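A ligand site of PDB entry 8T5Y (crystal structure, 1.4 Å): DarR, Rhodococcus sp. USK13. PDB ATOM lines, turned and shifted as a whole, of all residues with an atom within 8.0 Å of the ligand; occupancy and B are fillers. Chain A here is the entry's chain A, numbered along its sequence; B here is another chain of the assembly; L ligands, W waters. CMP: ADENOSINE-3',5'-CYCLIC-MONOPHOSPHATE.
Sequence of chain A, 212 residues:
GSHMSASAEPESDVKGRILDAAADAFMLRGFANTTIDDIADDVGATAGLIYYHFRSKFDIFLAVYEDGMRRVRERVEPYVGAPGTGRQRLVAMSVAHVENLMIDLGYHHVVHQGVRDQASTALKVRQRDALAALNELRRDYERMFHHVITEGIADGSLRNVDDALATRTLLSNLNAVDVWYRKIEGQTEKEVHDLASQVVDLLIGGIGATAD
Trp 180 touches the ligand. CE1 of Tyr 181 touches N6 of the ligand, at 3.1 Å. Ile 184 touches the ligand. Leu 195 touches the ligand (CD2 to N1, 3.6 Å). Of the 19 residues printed, 7 come within 4 Å of the ligand.
The guanidinium group of Arg 168 of chain B is in hydrogen-bond range of an oxygen (O2') of the ligand (2.9 Å). N of Arg 182 is in hydrogen-bond range of N7 of the ligand (3.1 Å). The backbone carbonyl oxygen (O) of Arg 182 sits at hydrogen-bond distance from a nitrogen (N6) of the ligand, 2.9 Å away. A nitrogen (N6) of the ligand lies within hydrogen-bond range of the side-chain amide oxygen of Gln 187 (2.9 Å).
Water W4 bridges a nitrogen (N7) of the ligand (3.0 Å) and the backbone carbonyl oxygen of Arg 182 (3.3 Å).
The backbone carbonyl oxygen (O) of Val 179 sits at hydrogen-bond distance from the guanidinium group (NH2) of Arg 182 (3.2 Å). The backbone carbonyl oxygen of Met 102 is in hydrogen-bond range of the side-chain hydroxyl of Tyr 181 (2.9 Å).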
ATOM      1  N   MET A 102      35.302 -17.038  24.274  1.00  0.00           N
ATOM      2  CA  MET A 102      34.002 -16.559  23.851  1.00  0.00           C
ATOM      3  C   MET A 102      34.111 -15.865  22.503  1.00  0.00           C
ATOM      4  O   MET A 102      33.191 -15.967  21.672  1.00  0.00           O
ATOM      5  CB  MET A 102      33.629 -15.611  24.986  1.00  0.00           C
ATOM      6  CG  MET A 102      33.003 -16.369  26.148  1.00  0.00           C
ATOM      7  SD  MET A 102      32.351 -15.259  27.381  1.00  0.00           S
ATOM      8  CE  MET A 102      31.763 -16.437  28.590  1.00  0.00           C
ATOM      9  N   LEU A 105      35.662 -18.888  19.607  1.00  0.00           N
ATOM     10  CA  LEU A 105      35.207 -20.180  20.103  1.00  0.00           C
ATOM     11  C   LEU A 105      35.684 -21.354  19.246  1.00  0.00           C
ATOM     12  O   LEU A 105      36.043 -22.404  19.777  1.00  0.00           O
ATOM     13  CB  LEU A 105      33.684 -20.188  20.188  1.00  0.00           C
ATOM     14  CG  LEU A 105      33.061 -21.386  20.896  1.00  0.00           C
ATOM     15  CD1 LEU A 105      33.567 -21.466  22.335  1.00  0.00           C
ATOM     16  CD2 LEU A 105      31.532 -21.282  20.861  1.00  0.00           C
ATOM     17  N   VAL A 177      33.533 -23.631  30.039  1.00  0.00           N
ATOM     18  CA  VAL A 177      32.559 -22.666  29.527  1.00  0.00           C
ATOM     19  C   VAL A 177      32.030 -23.099  28.172  1.00  0.00           C
ATOM     20  O   VAL A 177      30.881 -22.805  27.823  1.00  0.00           O
ATOM     21  CB  VAL A 177      33.201 -21.264  29.498  1.00  0.00           C
ATOM     22  CG1 VAL A 177      32.302 -20.252  28.787  1.00  0.00           C
ATOM     23  CG2 VAL A 177      33.519 -20.798  30.925  1.00  0.00           C
ATOM     24  N   VAL A 179      30.926 -25.820  27.223  1.00  0.00           N
ATOM     25  CA  VAL A 179      29.804 -26.751  27.291  1.00  0.00           C
ATOM     26  C   VAL A 179      28.509 -26.039  26.966  1.00  0.00           C
ATOM     27  O   VAL A 179      27.600 -26.613  26.348  1.00  0.00           O
ATOM     28  CB  VAL A 179      29.746 -27.441  28.672  1.00  0.00           C
ATOM     29  CG1 VAL A 179      28.458 -28.260  28.833  1.00  0.00           C
ATOM     30  CG2 VAL A 179      30.977 -28.305  28.868  1.00  0.00           C
ATOM     31  N   TRP A 180      28.375 -24.787  27.403  1.00  0.00           N
ATOM     32  CA  TRP A 180      27.121 -24.071  27.279  1.00  0.00           C
ATOM     33  C   TRP A 180      27.199 -22.796  26.459  1.00  0.00           C
ATOM     34  O   TRP A 180      26.168 -22.357  25.944  1.00  0.00           O
ATOM     35  CB  TRP A 180      26.524 -23.743  28.664  1.00  0.00           C
ATOM     36  CG  TRP A 180      27.447 -22.940  29.539  1.00  0.00           C
ATOM     37  CD1 TRP A 180      28.341 -23.418  30.462  1.00  0.00           C
ATOM     38  CD2 TRP A 180      27.606 -21.510  29.550  1.00  0.00           C
ATOM     39  NE1 TRP A 180      29.029 -22.393  31.060  1.00  0.00           N
ATOM     40  CE2 TRP A 180      28.596 -21.206  30.512  1.00  0.00           C
ATOM     41  CE3 TRP A 180      27.005 -20.456  28.848  1.00  0.00           C
ATOM     42  CZ2 TRP A 180      29.010 -19.885  30.785  1.00  0.00           C
ATOM     43  CZ3 TRP A 180      27.420 -19.143  29.127  1.00  0.00           C
ATOM     44  CH2 TRP A 180      28.393 -18.869  30.085  1.00  0.00           C
ATOM     45  N   TYR A 181      28.376 -22.187  26.328  1.00  0.00           N
ATOM     46  CA  TYR A 181      28.440 -20.896  25.665  1.00  0.00           C
ATOM     47  C   TYR A 181      28.312 -21.042  24.159  1.00  0.00           C
ATOM     48  O   TYR A 181      28.927 -21.923  23.542  1.00  0.00           O
ATOM     49  CB  TYR A 181      29.764 -20.192  25.984  1.00  0.00           C
ATOM     50  CG  TYR A 181      29.974 -18.925  25.182  1.00  0.00           C
ATOM     51  CD1 TYR A 181      29.439 -17.704  25.590  1.00  0.00           C
ATOM     52  CD2 TYR A 181      30.687 -18.959  23.988  1.00  0.00           C
ATOM     53  CE1 TYR A 181      29.650 -16.552  24.815  1.00  0.00           C
ATOM     54  CE2 TYR A 181      30.860 -17.827  23.226  1.00  0.00           C
ATOM     55  CZ  TYR A 181      30.369 -16.640  23.645  1.00  0.00           C
ATOM     56  OH  TYR A 181      30.573 -15.522  22.856  1.00  0.00           O
ATOM     57  N   ARG A 182      27.521 -20.169  23.564  1.00  0.00           N
ATOM     58  CA  ARG A 182      27.452 -20.032  22.114  1.00  0.00           C
ATOM     59  C   ARG A 182      27.518 -18.556  21.771  1.00  0.00           C
ATOM     60  O   ARG A 182      27.023 -17.708  22.518  1.00  0.00           O
ATOM     61  CB  ARG A 182      26.157 -20.640  21.552  1.00  0.00           C
ATOM     62  CG  ARG A 182      25.843 -22.042  22.072  1.00  0.00           C
ATOM     63  CD  ARG A 182      26.807 -23.089  21.504  1.00  0.00           C
ATOM     64  NE  ARG A 182      26.515 -24.439  21.954  1.00  0.00           N
ATOM     65  CZ  ARG A 182      27.164 -25.064  22.936  1.00  0.00           C
ATOM     66  NH1 ARG A 182      28.163 -24.474  23.580  1.00  0.00           N
ATOM     67  NH2 ARG A 182      26.796 -26.296  23.285  1.00  0.00           N
ATOM     68  N   LYS A 183      28.165 -18.242  20.661  1.00  0.00           N
ATOM     69  CA  LYS A 183      28.234 -16.853  20.220  1.00  0.00           C
ATOM     70  C   LYS A 183      26.844 -16.354  19.844  1.00  0.00           C
ATOM     71  O   LYS A 183      26.057 -17.062  19.218  1.00  0.00           O
ATOM     72  CB  LYS A 183      29.163 -16.717  19.024  1.00  0.00           C
ATOM     73  CG  LYS A 183      29.597 -15.288  18.725  1.00  0.00           C
ATOM     74  CD  LYS A 183      30.514 -15.251  17.509  1.00  0.00           C
ATOM     75  CE  LYS A 183      30.593 -13.861  16.901  1.00  0.00           C
ATOM     76  NZ  LYS A 183      31.748 -13.724  15.978  1.00  0.00           N
ATOM     77  N   ILE A 184      26.529 -15.125  20.259  1.00  0.00           N
ATOM     78  CA  ILE A 184      25.296 -14.460  19.870  1.00  0.00           C
ATOM     79  C   ILE A 184      25.670 -13.298  18.970  1.00  0.00           C
ATOM     80  O   ILE A 184      26.492 -12.447  19.348  1.00  0.00           O
ATOM     81  CB  ILE A 184      24.496 -13.983  21.098  1.00  0.00           C
ATOM     82  CG1 ILE A 184      24.082 -15.187  21.942  1.00  0.00           C
ATOM     83  CG2 ILE A 184      23.258 -13.201  20.632  1.00  0.00           C
ATOM     84  CD1 ILE A 184      23.426 -14.816  23.238  1.00  0.00           C
ATOM     85  N   GLU A 185      25.110 -13.264  17.764  1.00  0.00           N
ATOM     86  CA  GLU A 185      25.430 -12.193  16.827  1.00  0.00           C
ATOM     87  C   GLU A 185      24.997 -10.867  17.430  1.00  0.00           C
ATOM     88  O   GLU A 185      23.899 -10.736  17.963  1.00  0.00           O
ATOM     89  CB  GLU A 185      24.696 -12.423  15.507  1.00  0.00           C
ATOM     90  N   GLN A 187      26.191  -9.420  20.071  1.00  0.00           N
ATOM     91  CA  GLN A 187      26.579  -9.214  21.454  1.00  0.00           C
ATOM     92  C   GLN A 187      27.844  -8.375  21.458  1.00  0.00           C
ATOM     93  O   GLN A 187      28.782  -8.645  20.705  1.00  0.00           O
ATOM     94  CB  GLN A 187      26.852 -10.569  22.123  1.00  0.00           C
ATOM     95  CG  GLN A 187      26.640 -10.558  23.632  1.00  0.00           C
ATOM     96  CD  GLN A 187      26.742 -11.943  24.249  1.00  0.00           C
ATOM     97  OE1 GLN A 187      27.272 -12.876  23.641  1.00  0.00           O
ATOM     98  NE2 GLN A 187      26.216 -12.080  25.460  1.00  0.00           N
ATOM     99  N   GLU A 191      29.674  -6.705  26.582  1.00  0.00           N
ATOM    100  CA  GLU A 191      28.773  -7.759  27.029  1.00  0.00           C
ATOM    101  C   GLU A 191      29.497  -9.088  27.157  1.00  0.00           C
ATOM    102  O   GLU A 191      29.262  -9.841  28.125  1.00  0.00           O
ATOM    103  CB  GLU A 191      27.605  -7.874  26.039  1.00  0.00           C
ATOM    104  CG  GLU A 191      26.617  -6.713  26.162  1.00  0.00           C
ATOM    105  CD  GLU A 191      25.414  -6.860  25.240  1.00  0.00           C
ATOM    106  OE1 GLU A 191      25.618  -7.170  24.046  1.00  0.00           O
ATOM    107  OE2 GLU A 191      24.265  -6.651  25.699  1.00  0.00           O
ATOM    108  N   VAL A 192      30.379  -9.408  26.210  1.00  0.00           N
ATOM    109  CA  VAL A 192      31.153 -10.640  26.311  1.00  0.00           C
ATOM    110  C   VAL A 192      32.143 -10.559  27.466  1.00  0.00           C
ATOM    111  O   VAL A 192      32.247 -11.493  28.279  1.00  0.00           O
ATOM    112  CB  VAL A 192      31.832 -10.956  24.966  1.00  0.00           C
ATOM    113  CG1 VAL A 192      32.861 -12.073  25.124  1.00  0.00           C
ATOM    114  CG2 VAL A 192      30.778 -11.281  23.910  1.00  0.00           C
ATOM    115  N   LEU A 195      30.191 -11.088  30.696  1.00  0.00           N
ATOM    116  CA  LEU A 195      29.872 -12.490  30.942  1.00  0.00           C
ATOM    117  C   LEU A 195      31.090 -13.269  31.417  1.00  0.00           C
ATOM    118  O   LEU A 195      31.018 -14.052  32.381  1.00  0.00           O
ATOM    119  CB  LEU A 195      29.235 -13.114  29.699  1.00  0.00           C
ATOM    120  CG  LEU A 195      28.743 -14.549  29.835  1.00  0.00           C
ATOM    121  CD1 LEU A 195      27.598 -14.637  30.832  1.00  0.00           C
ATOM    122  CD2 LEU A 195      28.321 -15.058  28.470  1.00  0.00           C
ATOM    123  N   GLN A 198      31.689 -12.485  35.026  1.00  0.00           N
ATOM    124  CA  GLN A 198      30.760 -13.171  35.913  1.00  0.00           C
ATOM    125  C   GLN A 198      31.167 -14.625  36.111  1.00  0.00           C
ATOM    126  O   GLN A 198      31.081 -15.158  37.222  1.00  0.00           O
ATOM    127  CB  GLN A 198      29.358 -13.135  35.326  1.00  0.00           C
ATOM    128  CG  GLN A 198      28.630 -11.849  35.428  1.00  0.00           C
ATOM    129  CD  GLN A 198      27.230 -12.028  34.897  1.00  0.00           C
ATOM    130  OE1 GLN A 198      27.031 -12.100  33.701  1.00  0.00           O
ATOM    131  NE2 GLN A 198      26.261 -12.113  35.810  1.00  0.00           N
ATOM    132  N   ASP B 162      23.737 -14.967  39.647  1.00  0.00           N
ATOM    133  CA  ASP B 162      22.690 -15.401  38.734  1.00  0.00           C
ATOM    134  C   ASP B 162      22.535 -16.916  38.851  1.00  0.00           C
ATOM    135  O   ASP B 162      23.515 -17.666  38.697  1.00  0.00           O
ATOM    136  CB  ASP B 162      23.066 -15.048  37.311  1.00  0.00           C
ATOM    137  CG  ASP B 162      21.991 -15.434  36.331  1.00  0.00           C
ATOM    138  OD1 ASP B 162      21.022 -14.663  36.183  1.00  0.00           O
ATOM    139  OD2 ASP B 162      22.064 -16.532  35.757  1.00  0.00           O
ATOM    140  N   ALA B 164      20.912 -19.195  37.002  1.00  0.00           N
ATOM    141  CA  ALA B 164      21.085 -19.981  35.784  1.00  0.00           C
ATOM    142  C   ALA B 164      22.564 -20.107  35.428  1.00  0.00           C
ATOM    143  O   ALA B 164      23.045 -21.217  35.127  1.00  0.00           O
ATOM    144  CB  ALA B 164      20.297 -19.366  34.629  1.00  0.00           C
ATOM    145  N   LEU B 165      23.295 -18.990  35.477  1.00  0.00           N
ATOM    146  CA  LEU B 165      24.724 -19.057  35.202  1.00  0.00           C
ATOM    147  C   LEU B 165      25.436 -19.919  36.232  1.00  0.00           C
ATOM    148  O   LEU B 165      26.301 -20.732  35.893  1.00  0.00           O
ATOM    149  CB  LEU B 165      25.338 -17.663  35.201  1.00  0.00           C
ATOM    150  CG  LEU B 165      26.855 -17.616  34.900  1.00  0.00           C
ATOM    151  CD1 LEU B 165      27.168 -18.163  33.490  1.00  0.00           C
ATOM    152  CD2 LEU B 165      27.397 -16.200  35.076  1.00  0.00           C
ATOM    153  N   ARG B 168      24.739 -23.668  35.416  1.00  0.00           N
ATOM    154  CA  ARG B 168      25.469 -24.132  34.240  1.00  0.00           C
ATOM    155  C   ARG B 168      26.959 -24.217  34.514  1.00  0.00           C
ATOM    156  O   ARG B 168      27.611 -25.167  34.096  1.00  0.00           O
ATOM    157  CB  ARG B 168      25.215 -23.195  33.055  1.00  0.00           C
ATOM    158  CG  ARG B 168      23.861 -23.384  32.447  1.00  0.00           C
ATOM    159  CD  ARG B 168      23.768 -22.647  31.130  1.00  0.00           C
ATOM    160  NE  ARG B 168      23.518 -21.234  31.354  1.00  0.00           N
ATOM    161  CZ  ARG B 168      22.313 -20.703  31.471  1.00  0.00           C
ATOM    162  NH1 ARG B 168      21.218 -21.464  31.391  1.00  0.00           N
ATOM    163  NH2 ARG B 168      22.191 -19.400  31.670  1.00  0.00           N
HETATM  164  P   CMP L   1      20.035 -22.079  26.345  1.00  0.00           P
HETATM  165  O1P CMP L   1      18.674 -22.612  26.737  1.00  0.00           O
HETATM  166  O2P CMP L   1      20.367 -21.953  24.878  1.00  0.00           O
HETATM  167  O5' CMP L   1      21.129 -23.074  26.973  1.00  0.00           O
HETATM  168  C5' CMP L   1      22.437 -22.633  27.333  1.00  0.00           C
HETATM  169  C4' CMP L   1      22.344 -21.273  27.962  1.00  0.00           C
HETATM  170  O4' CMP L   1      23.626 -20.637  28.147  1.00  0.00           O
HETATM  171  C3' CMP L   1      21.591 -20.275  27.130  1.00  0.00           C
HETATM  172  O3' CMP L   1      20.227 -20.615  27.026  1.00  0.00           O
HETATM  173  C2' CMP L   1      21.948 -18.967  27.818  1.00  0.00           C
HETATM  174  O2' CMP L   1      21.226 -18.820  29.022  1.00  0.00           O
HETATM  175  C1' CMP L   1      23.425 -19.232  28.149  1.00  0.00           C
HETATM  176  N9  CMP L   1      24.305 -18.638  27.131  1.00  0.00           N
HETATM  177  C8  CMP L   1      24.918 -19.275  26.115  1.00  0.00           C
HETATM  178  N7  CMP L   1      25.627 -18.412  25.339  1.00  0.00           N
HETATM  179  C5  CMP L   1      25.439 -17.182  25.861  1.00  0.00           C
HETATM  180  C6  CMP L   1      25.898 -15.819  25.546  1.00  0.00           C
HETATM  181  N6  CMP L   1      26.686 -15.611  24.469  1.00  0.00           N
HETATM  182  N1  CMP L   1      25.482 -14.815  26.335  1.00  0.00           N
HETATM  183  C2  CMP L   1      24.682 -15.016  27.407  1.00  0.00           C
HETATM  184  N3  CMP L   1      24.223 -16.228  27.768  1.00  0.00           N
HETATM  185  C4  CMP L   1      24.570 -17.331  27.043  1.00  0.00           C
HETATM  186  O   HOH W   1      24.238 -23.731  24.674  1.00  0.00           O
HETATM  187  O   HOH W   2      22.590 -21.320  23.468  1.00  0.00           O
HETATM  188  O   HOH W   3      24.623 -18.774  31.351  1.00  0.00           O
HETATM  189  O   HOH W   4      23.776 -18.368  22.954  1.00  0.00           O
